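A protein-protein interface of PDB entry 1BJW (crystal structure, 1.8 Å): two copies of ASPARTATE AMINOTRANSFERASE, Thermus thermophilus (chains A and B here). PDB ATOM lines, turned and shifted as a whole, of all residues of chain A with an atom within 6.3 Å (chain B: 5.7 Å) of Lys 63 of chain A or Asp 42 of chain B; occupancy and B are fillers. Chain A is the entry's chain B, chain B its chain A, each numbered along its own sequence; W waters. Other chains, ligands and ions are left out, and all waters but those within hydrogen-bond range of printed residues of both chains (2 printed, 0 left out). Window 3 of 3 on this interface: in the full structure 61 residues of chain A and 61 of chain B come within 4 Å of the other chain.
The backbone NH (N) of Tyr 64 of chain A is in hydrogen-bond range of the side-chain carboxylate (OE1) of Glu 40 of chain B, at 2.9 Å.
The backbone carbonyl oxygen of Pro 41 of chain B sits at hydrogen-bond distance from the side-chain amino group of Lys 63 of chain A, 2.7 Å away.
The backbone carbonyl oxygen of Phe 43 of chain B lies within hydrogen-bond range of the side-chain amino group of Lys 63 of chain A, at 2.8 Å.
The side-chain hydroxyl (OG1) of Thr 62 of chain A sits at hydrogen-bond distance from the side-chain carboxylate (OD1) of Asp 44 of chain B (2.9 Å).
O of Thr 62 of chain A lies within hydrogen-bond range of N of Gly 240 of chain B, at 2.9 Å.
N of Thr 269 of chain A is in hydrogen-bond range of O of Gly 240 of chain B, 2.8 Å away.
OE1 of Glu 40 of chain B is in hydrogen-bond range of OG1 of Thr 239 of chain B (2.7 Å).
OD1 of Asp 42 of chain B lies within salt-bridge range of NH1 of Arg 299 of chain B, at 2.7 Å.
O of Lys 63 of chain A sits at hydrogen-bond distance from OG1 of Thr 269 of chain A (2.6 Å).
Among the printed residues, merely in contact across the chains: Gly 60 of chain A with Asp 44 of chain B, Thr 62 of chain A with Thr 45 of chain B, Thr 62 of chain A with Thr 239 of chain B, Lys 63 of chain A with Glu 40 of chain B, Lys 63 of chain A with Asp 42 of chain B, Lys 63 of chain A with Thr 239 of chain B, Lys 63 of chain A with Gly 240 of chain B and Tyr 64 of chain A with Thr 239 of chain B.
Of the printed residues of chain B, Gly 60 of chain A touches Asp 44.
Printed residues of chain B within 4 Å of Lys 63 of chain A: Glu 40, Pro 41, Asp 42, Phe 43, Thr 239 and Gly 240.
Of the printed residues of chain B, Thr 269 of chain A touches Gly 240 (2.8 Å).
Printed residues of chain A within 4 Å of Pro 41 of chain B: Lys 63 (2.7 Å).
Asp 42 of chain B touches just one residue of chain A: Lys 63.
Of the printed residues of chain A, Phe 43 of chain B touches Lys 63 (2.8 Å).
Of the printed residues of chain A, Thr 45 of chain B touches Thr 62 (3.3 Å).
Ala 237 of chain B touches none of the printed residues of chain A.
Ala 365 of chain B touches none of the printed residues of chain A.
The nearest residue of chain B that does not touch Lys 63 of chain A is Asp 44 of chain B (4.4 Å).
The nearest printed residue of chain A that does not touch Gly 240 of chain B is Tyr 64 of chain A (4.1 Å).
Printed residues of chain A that touch a printed residue of chain B: Gly 60, Thr 62, Lys 63, Tyr 64 and Thr 269.
Along chain A the printed residues that touch a printed residue of chain B span positions 60 to 269.
No position is printed for both chains.
Of the 14 pairs that touch across the chains among the printed residues, none has its exchanged pair printed and touching as well.
Water W1 lies within hydrogen-bond range of OG1 of Thr 62 of chain A, O of Ala 237 of chain B, NZ of Lys 63 of chain A and O of Phe 43 of chain B.
Water W2 bridges the side-chain carboxylate (OE2) of Glu 40 of chain B and the backbone carbonyl oxygen (O) of Tyr 64 of chain A.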
ATOM      1  N   GLY A  60     -10.001   0.075 -12.378  1.00  0.00           N
ATOM      2  CA  GLY A  60     -11.218   0.856 -12.522  1.00  0.00           C
ATOM      3  C   GLY A  60     -12.497   0.218 -12.045  1.00  0.00           C
ATOM      4  O   GLY A  60     -13.522   0.354 -12.695  1.00  0.00           O
ATOM      5  N   LYS A  61     -12.432  -0.508 -10.932  1.00  0.00           N
ATOM      6  CA  LYS A  61     -13.610  -1.142 -10.338  1.00  0.00           C
ATOM      7  C   LYS A  61     -14.238  -0.090  -9.420  1.00  0.00           C
ATOM      8  O   LYS A  61     -14.218  -0.198  -8.179  1.00  0.00           O
ATOM      9  CB  LYS A  61     -13.172  -2.363  -9.568  1.00  0.00           C
ATOM     10  CG  LYS A  61     -12.672  -3.443 -10.483  1.00  0.00           C
ATOM     11  CD  LYS A  61     -11.968  -4.506  -9.688  1.00  0.00           C
ATOM     12  CE  LYS A  61     -11.874  -5.815 -10.449  1.00  0.00           C
ATOM     13  NZ  LYS A  61     -10.988  -6.811  -9.723  1.00  0.00           N
ATOM     14  N   THR A  62     -14.795   0.934 -10.066  1.00  0.00           N
ATOM     15  CA  THR A  62     -15.353   2.090  -9.388  1.00  0.00           C
ATOM     16  C   THR A  62     -16.824   2.322  -9.679  1.00  0.00           C
ATOM     17  O   THR A  62     -17.348   3.408  -9.396  1.00  0.00           O
ATOM     18  CB  THR A  62     -14.552   3.332  -9.801  1.00  0.00           C
ATOM     19  OG1 THR A  62     -14.671   3.503 -11.220  1.00  0.00           O
ATOM     20  CG2 THR A  62     -13.069   3.157  -9.462  1.00  0.00           C
ATOM     21  N   LYS A  63     -17.502   1.280 -10.154  1.00  0.00           N
ATOM     22  CA  LYS A  63     -18.907   1.352 -10.522  1.00  0.00           C
ATOM     23  C   LYS A  63     -19.832   0.725  -9.482  1.00  0.00           C
ATOM     24  O   LYS A  63     -19.377   0.048  -8.564  1.00  0.00           O
ATOM     25  CB  LYS A  63     -19.119   0.640 -11.877  1.00  0.00           C
ATOM     26  CG  LYS A  63     -18.128   1.022 -12.964  1.00  0.00           C
ATOM     27  CD  LYS A  63     -18.280   2.470 -13.321  1.00  0.00           C
ATOM     28  CE  LYS A  63     -17.318   2.931 -14.412  1.00  0.00           C
ATOM     29  NZ  LYS A  63     -17.645   4.325 -14.836  1.00  0.00           N
ATOM     30  N   TYR A  64     -21.133   0.967  -9.630  1.00  0.00           N
ATOM     31  CA  TYR A  64     -22.145   0.410  -8.731  1.00  0.00           C
ATOM     32  C   TYR A  64     -22.043  -1.105  -8.681  1.00  0.00           C
ATOM     33  O   TYR A  64     -21.898  -1.756  -9.712  1.00  0.00           O
ATOM     34  CB  TYR A  64     -23.558   0.727  -9.226  1.00  0.00           C
ATOM     35  CG  TYR A  64     -24.032   2.137  -8.999  1.00  0.00           C
ATOM     36  CD1 TYR A  64     -23.991   2.719  -7.723  1.00  0.00           C
ATOM     37  CD2 TYR A  64     -24.594   2.873 -10.039  1.00  0.00           C
ATOM     38  CE1 TYR A  64     -24.508   4.000  -7.499  1.00  0.00           C
ATOM     39  CE2 TYR A  64     -25.122   4.164  -9.824  1.00  0.00           C
ATOM     40  CZ  TYR A  64     -25.077   4.716  -8.549  1.00  0.00           C
ATOM     41  OH  TYR A  64     -25.628   5.957  -8.317  1.00  0.00           O
ATOM     42  N   ALA A  65     -22.143  -1.657  -7.471  1.00  0.00           N
ATOM     43  CA  ALA A  65     -22.127  -3.112  -7.234  1.00  0.00           C
ATOM     44  C   ALA A  65     -23.593  -3.540  -6.965  1.00  0.00           C
ATOM     45  O   ALA A  65     -24.436  -2.691  -6.645  1.00  0.00           O
ATOM     46  CB  ALA A  65     -21.257  -3.428  -6.000  1.00  0.00           C
ATOM     47  N   ILE A  70     -20.979  -7.845  -4.466  1.00  0.00           N
ATOM     48  CA  ILE A  70     -20.301  -8.406  -5.613  1.00  0.00           C
ATOM     49  C   ILE A  70     -20.405  -9.942  -5.531  1.00  0.00           C
ATOM     50  O   ILE A  70     -20.162 -10.530  -4.492  1.00  0.00           O
ATOM     51  CB  ILE A  70     -18.846  -7.806  -5.592  1.00  0.00           C
ATOM     52  CG1 ILE A  70     -18.575  -7.079  -6.876  1.00  0.00           C
ATOM     53  CG2 ILE A  70     -17.774  -8.701  -5.036  1.00  0.00           C
ATOM     54  CD1 ILE A  70     -19.233  -5.768  -6.887  1.00  0.00           C
ATOM     55  N   THR A 269     -17.432  -0.202  -3.757  1.00  0.00           N
ATOM     56  CA  THR A 269     -16.883  -1.297  -4.594  1.00  0.00           C
ATOM     57  C   THR A 269     -15.419  -1.684  -4.350  1.00  0.00           C
ATOM     58  O   THR A 269     -15.077  -2.866  -4.428  1.00  0.00           O
ATOM     59  CB  THR A 269     -17.109  -0.988  -6.083  1.00  0.00           C
ATOM     60  OG1 THR A 269     -18.512  -0.815  -6.281  1.00  0.00           O
ATOM     61  CG2 THR A 269     -16.618  -2.123  -6.981  1.00  0.00           C
ATOM     62  N   GLU B  40     -25.020   5.441 -14.646  1.00  0.00           N
ATOM     63  CA  GLU B  40     -23.767   5.969 -14.142  1.00  0.00           C
ATOM     64  C   GLU B  40     -22.839   6.338 -15.302  1.00  0.00           C
ATOM     65  O   GLU B  40     -22.994   5.826 -16.413  1.00  0.00           O
ATOM     66  CB  GLU B  40     -23.113   4.915 -13.227  1.00  0.00           C
ATOM     67  CG  GLU B  40     -22.842   3.578 -13.910  1.00  0.00           C
ATOM     68  CD  GLU B  40     -22.385   2.461 -12.979  1.00  0.00           C
ATOM     69  OE1 GLU B  40     -21.943   2.728 -11.848  1.00  0.00           O
ATOM     70  OE2 GLU B  40     -22.419   1.298 -13.411  1.00  0.00           O
ATOM     71  N   PRO B  41     -21.874   7.241 -15.064  1.00  0.00           N
ATOM     72  CA  PRO B  41     -20.951   7.631 -16.141  1.00  0.00           C
ATOM     73  C   PRO B  41     -20.144   6.448 -16.670  1.00  0.00           C
ATOM     74  O   PRO B  41     -19.876   5.496 -15.936  1.00  0.00           O
ATOM     75  CB  PRO B  41     -20.039   8.642 -15.459  1.00  0.00           C
ATOM     76  CG  PRO B  41     -20.943   9.231 -14.354  1.00  0.00           C
ATOM     77  CD  PRO B  41     -21.636   8.017 -13.832  1.00  0.00           C
ATOM     78  N   ASP B  42     -19.753   6.516 -17.942  1.00  0.00           N
ATOM     79  CA  ASP B  42     -18.943   5.464 -18.564  1.00  0.00           C
ATOM     80  C   ASP B  42     -17.450   5.693 -18.242  1.00  0.00           C
ATOM     81  O   ASP B  42     -16.645   4.747 -18.181  1.00  0.00           O
ATOM     82  CB  ASP B  42     -19.186   5.436 -20.075  1.00  0.00           C
ATOM     83  CG  ASP B  42     -19.041   6.813 -20.722  1.00  0.00           C
ATOM     84  OD1 ASP B  42     -19.863   7.721 -20.434  1.00  0.00           O
ATOM     85  OD2 ASP B  42     -18.091   6.976 -21.522  1.00  0.00           O
ATOM     86  N   PHE B  43     -17.109   6.953 -17.990  1.00  0.00           N
ATOM     87  CA  PHE B  43     -15.756   7.345 -17.631  1.00  0.00           C
ATOM     88  C   PHE B  43     -15.308   6.752 -16.302  1.00  0.00           C
ATOM     89  O   PHE B  43     -16.129   6.552 -15.411  1.00  0.00           O
ATOM     90  CB  PHE B  43     -15.713   8.851 -17.487  1.00  0.00           C
ATOM     91  CG  PHE B  43     -16.096   9.568 -18.722  1.00  0.00           C
ATOM     92  CD1 PHE B  43     -15.151   9.824 -19.704  1.00  0.00           C
ATOM     93  CD2 PHE B  43     -17.409   9.948 -18.938  1.00  0.00           C
ATOM     94  CE1 PHE B  43     -15.512  10.448 -20.893  1.00  0.00           C
ATOM     95  CE2 PHE B  43     -17.781  10.575 -20.128  1.00  0.00           C
ATOM     96  CZ  PHE B  43     -16.828  10.821 -21.104  1.00  0.00           C
ATOM     97  N   ASP B  44     -14.015   6.468 -16.177  1.00  0.00           N
ATOM     98  CA  ASP B  44     -13.476   5.954 -14.917  1.00  0.00           C
ATOM     99  C   ASP B  44     -13.266   7.176 -14.019  1.00  0.00           C
ATOM    100  O   ASP B  44     -13.264   8.308 -14.512  1.00  0.00           O
ATOM    101  CB  ASP B  44     -12.144   5.247 -15.134  1.00  0.00           C
ATOM    102  CG  ASP B  44     -11.742   4.357 -13.945  1.00  0.00           C
ATOM    103  OD1 ASP B  44     -12.513   4.220 -12.965  1.00  0.00           O
ATOM    104  OD2 ASP B  44     -10.644   3.768 -13.986  1.00  0.00           O
ATOM    105  N   THR B  45     -13.127   6.978 -12.709  1.00  0.00           N
ATOM    106  CA  THR B  45     -12.918   8.131 -11.853  1.00  0.00           C
ATOM    107  C   THR B  45     -11.550   8.709 -12.115  1.00  0.00           C
ATOM    108  O   THR B  45     -10.600   7.971 -12.348  1.00  0.00           O
ATOM    109  CB  THR B  45     -13.219   7.879 -10.323  1.00  0.00           C
ATOM    110  OG1 THR B  45     -12.142   8.331  -9.494  1.00  0.00           O
ATOM    111  CG2 THR B  45     -13.570   6.493 -10.047  1.00  0.00           C
ATOM    112  N   ALA B 237     -17.739  10.657 -11.758  1.00  0.00           N
ATOM    113  CA  ALA B 237     -17.729   9.244 -12.065  1.00  0.00           C
ATOM    114  C   ALA B 237     -17.244   8.449 -10.831  1.00  0.00           C
ATOM    115  O   ALA B 237     -16.287   7.659 -10.884  1.00  0.00           O
ATOM    116  CB  ALA B 237     -16.844   8.980 -13.299  1.00  0.00           C
ATOM    117  N   THR B 239     -19.632   6.637  -8.745  1.00  0.00           N
ATOM    118  CA  THR B 239     -20.793   5.913  -8.247  1.00  0.00           C
ATOM    119  C   THR B 239     -20.476   4.772  -7.261  1.00  0.00           C
ATOM    120  O   THR B 239     -21.157   4.599  -6.253  1.00  0.00           O
ATOM    121  CB  THR B 239     -21.666   5.345  -9.395  1.00  0.00           C
ATOM    122  OG1 THR B 239     -20.851   4.534 -10.237  1.00  0.00           O
ATOM    123  CG2 THR B 239     -22.316   6.468 -10.211  1.00  0.00           C
ATOM    124  N   GLY B 240     -19.433   4.008  -7.534  1.00  0.00           N
ATOM    125  CA  GLY B 240     -19.094   2.899  -6.667  1.00  0.00           C
ATOM    126  C   GLY B 240     -18.406   3.278  -5.385  1.00  0.00           C
ATOM    127  O   GLY B 240     -18.222   2.419  -4.549  1.00  0.00           O
ATOM    128  N   TYR B 296     -20.688  14.262 -23.308  1.00  0.00           N
ATOM    129  CA  TYR B 296     -22.142  14.066 -23.207  1.00  0.00           C
ATOM    130  C   TYR B 296     -22.911  14.917 -24.225  1.00  0.00           C
ATOM    131  O   TYR B 296     -23.882  14.449 -24.785  1.00  0.00           O
ATOM    132  CB  TYR B 296     -22.682  14.361 -21.801  1.00  0.00           C
ATOM    133  CG  TYR B 296     -22.161  13.446 -20.706  1.00  0.00           C
ATOM    134  CD1 TYR B 296     -22.127  12.060 -20.874  1.00  0.00           C
ATOM    135  CD2 TYR B 296     -21.648  13.978 -19.523  1.00  0.00           C
ATOM    136  CE1 TYR B 296     -21.583  11.224 -19.890  1.00  0.00           C
ATOM    137  CE2 TYR B 296     -21.104  13.151 -18.537  1.00  0.00           C
ATOM    138  CZ  TYR B 296     -21.069  11.785 -18.725  1.00  0.00           C
ATOM    139  OH  TYR B 296     -20.478  10.986 -17.773  1.00  0.00           O
ATOM    140  N   ARG B 299     -22.678  13.318 -27.614  1.00  0.00           N
ATOM    141  CA  ARG B 299     -23.502  12.129 -27.635  1.00  0.00           C
ATOM    142  C   ARG B 299     -24.997  12.388 -27.653  1.00  0.00           C
ATOM    143  O   ARG B 299     -25.756  11.664 -28.310  1.00  0.00           O
ATOM    144  CB  ARG B 299     -23.132  11.221 -26.478  1.00  0.00           C
ATOM    145  CG  ARG B 299     -21.692  10.775 -26.485  1.00  0.00           C
ATOM    146  CD  ARG B 299     -21.430  10.020 -25.196  1.00  0.00           C
ATOM    147  NE  ARG B 299     -20.048   9.620 -25.022  1.00  0.00           N
ATOM    148  CZ  ARG B 299     -19.559   9.154 -23.872  1.00  0.00           C
ATOM    149  NH1 ARG B 299     -20.350   9.039 -22.797  1.00  0.00           N
ATOM    150  NH2 ARG B 299     -18.293   8.806 -23.794  1.00  0.00           N
ATOM    151  N   TYR B 364     -27.294   8.020 -22.500  1.00  0.00           N
ATOM    152  CA  TYR B 364     -26.167   8.231 -23.399  1.00  0.00           C
ATOM    153  C   TYR B 364     -24.794   8.262 -22.718  1.00  0.00           C
ATOM    154  O   TYR B 364     -23.850   8.878 -23.214  1.00  0.00           O
ATOM    155  CB  TYR B 364     -26.391   9.361 -24.431  1.00  0.00           C
ATOM    156  CG  TYR B 364     -26.847  10.670 -23.891  1.00  0.00           C
ATOM    157  CD1 TYR B 364     -28.203  10.948 -23.749  1.00  0.00           C
ATOM    158  CD2 TYR B 364     -25.920  11.653 -23.558  1.00  0.00           C
ATOM    159  CE1 TYR B 364     -28.632  12.180 -23.284  1.00  0.00           C
ATOM    160  CE2 TYR B 364     -26.323  12.892 -23.104  1.00  0.00           C
ATOM    161  CZ  TYR B 364     -27.679  13.159 -22.964  1.00  0.00           C
ATOM    162  OH  TYR B 364     -28.077  14.416 -22.532  1.00  0.00           O
ATOM    163  N   ALA B 365     -24.686   7.548 -21.590  1.00  0.00           N
ATOM    164  CA  ALA B 365     -23.422   7.418 -20.885  1.00  0.00           C
ATOM    165  C   ALA B 365     -22.771   6.130 -21.415  1.00  0.00           C
ATOM    166  O   ALA B 365     -22.637   5.153 -20.687  1.00  0.00           O
ATOM    167  CB  ALA B 365     -23.651   7.312 -19.388  1.00  0.00           C
ATOM    168  N   THR B 366     -22.502   6.107 -22.727  1.00  0.00           N
ATOM    169  CA  THR B 366     -21.854   4.989 -23.450  1.00  0.00           C
ATOM    170  C   THR B 366     -21.197   5.619 -24.693  1.00  0.00           C
ATOM    171  O   THR B 366     -21.496   6.768 -25.029  1.00  0.00           O
ATOM    172  CB  THR B 366     -22.854   3.890 -23.909  1.00  0.00           C
ATOM    173  OG1 THR B 366     -23.603   4.345 -25.046  1.00  0.00           O
ATOM    174  CG2 THR B 366     -23.845   3.578 -22.812  1.00  0.00           C
ATOM    175  N   SER B 367     -20.322   4.889 -25.378  1.00  0.00           N
ATOM    176  CA  SER B 367     -19.638   5.447 -26.545  1.00  0.00           C
ATOM    177  C   SER B 367     -20.531   5.825 -27.722  1.00  0.00           C
ATOM    178  O   SER B 367     -21.648   5.354 -27.844  1.00  0.00           O
ATOM    179  CB  SER B 367     -18.548   4.497 -27.046  1.00  0.00           C
ATOM    180  OG  SER B 367     -19.076   3.250 -27.460  1.00  0.00           O
HETATM  181  O   HOH W   1     -16.305   5.239 -12.327  1.00  0.00           O
HETATM  182  O   HOH W   2     -22.339  -1.248 -12.426  1.00  0.00           O
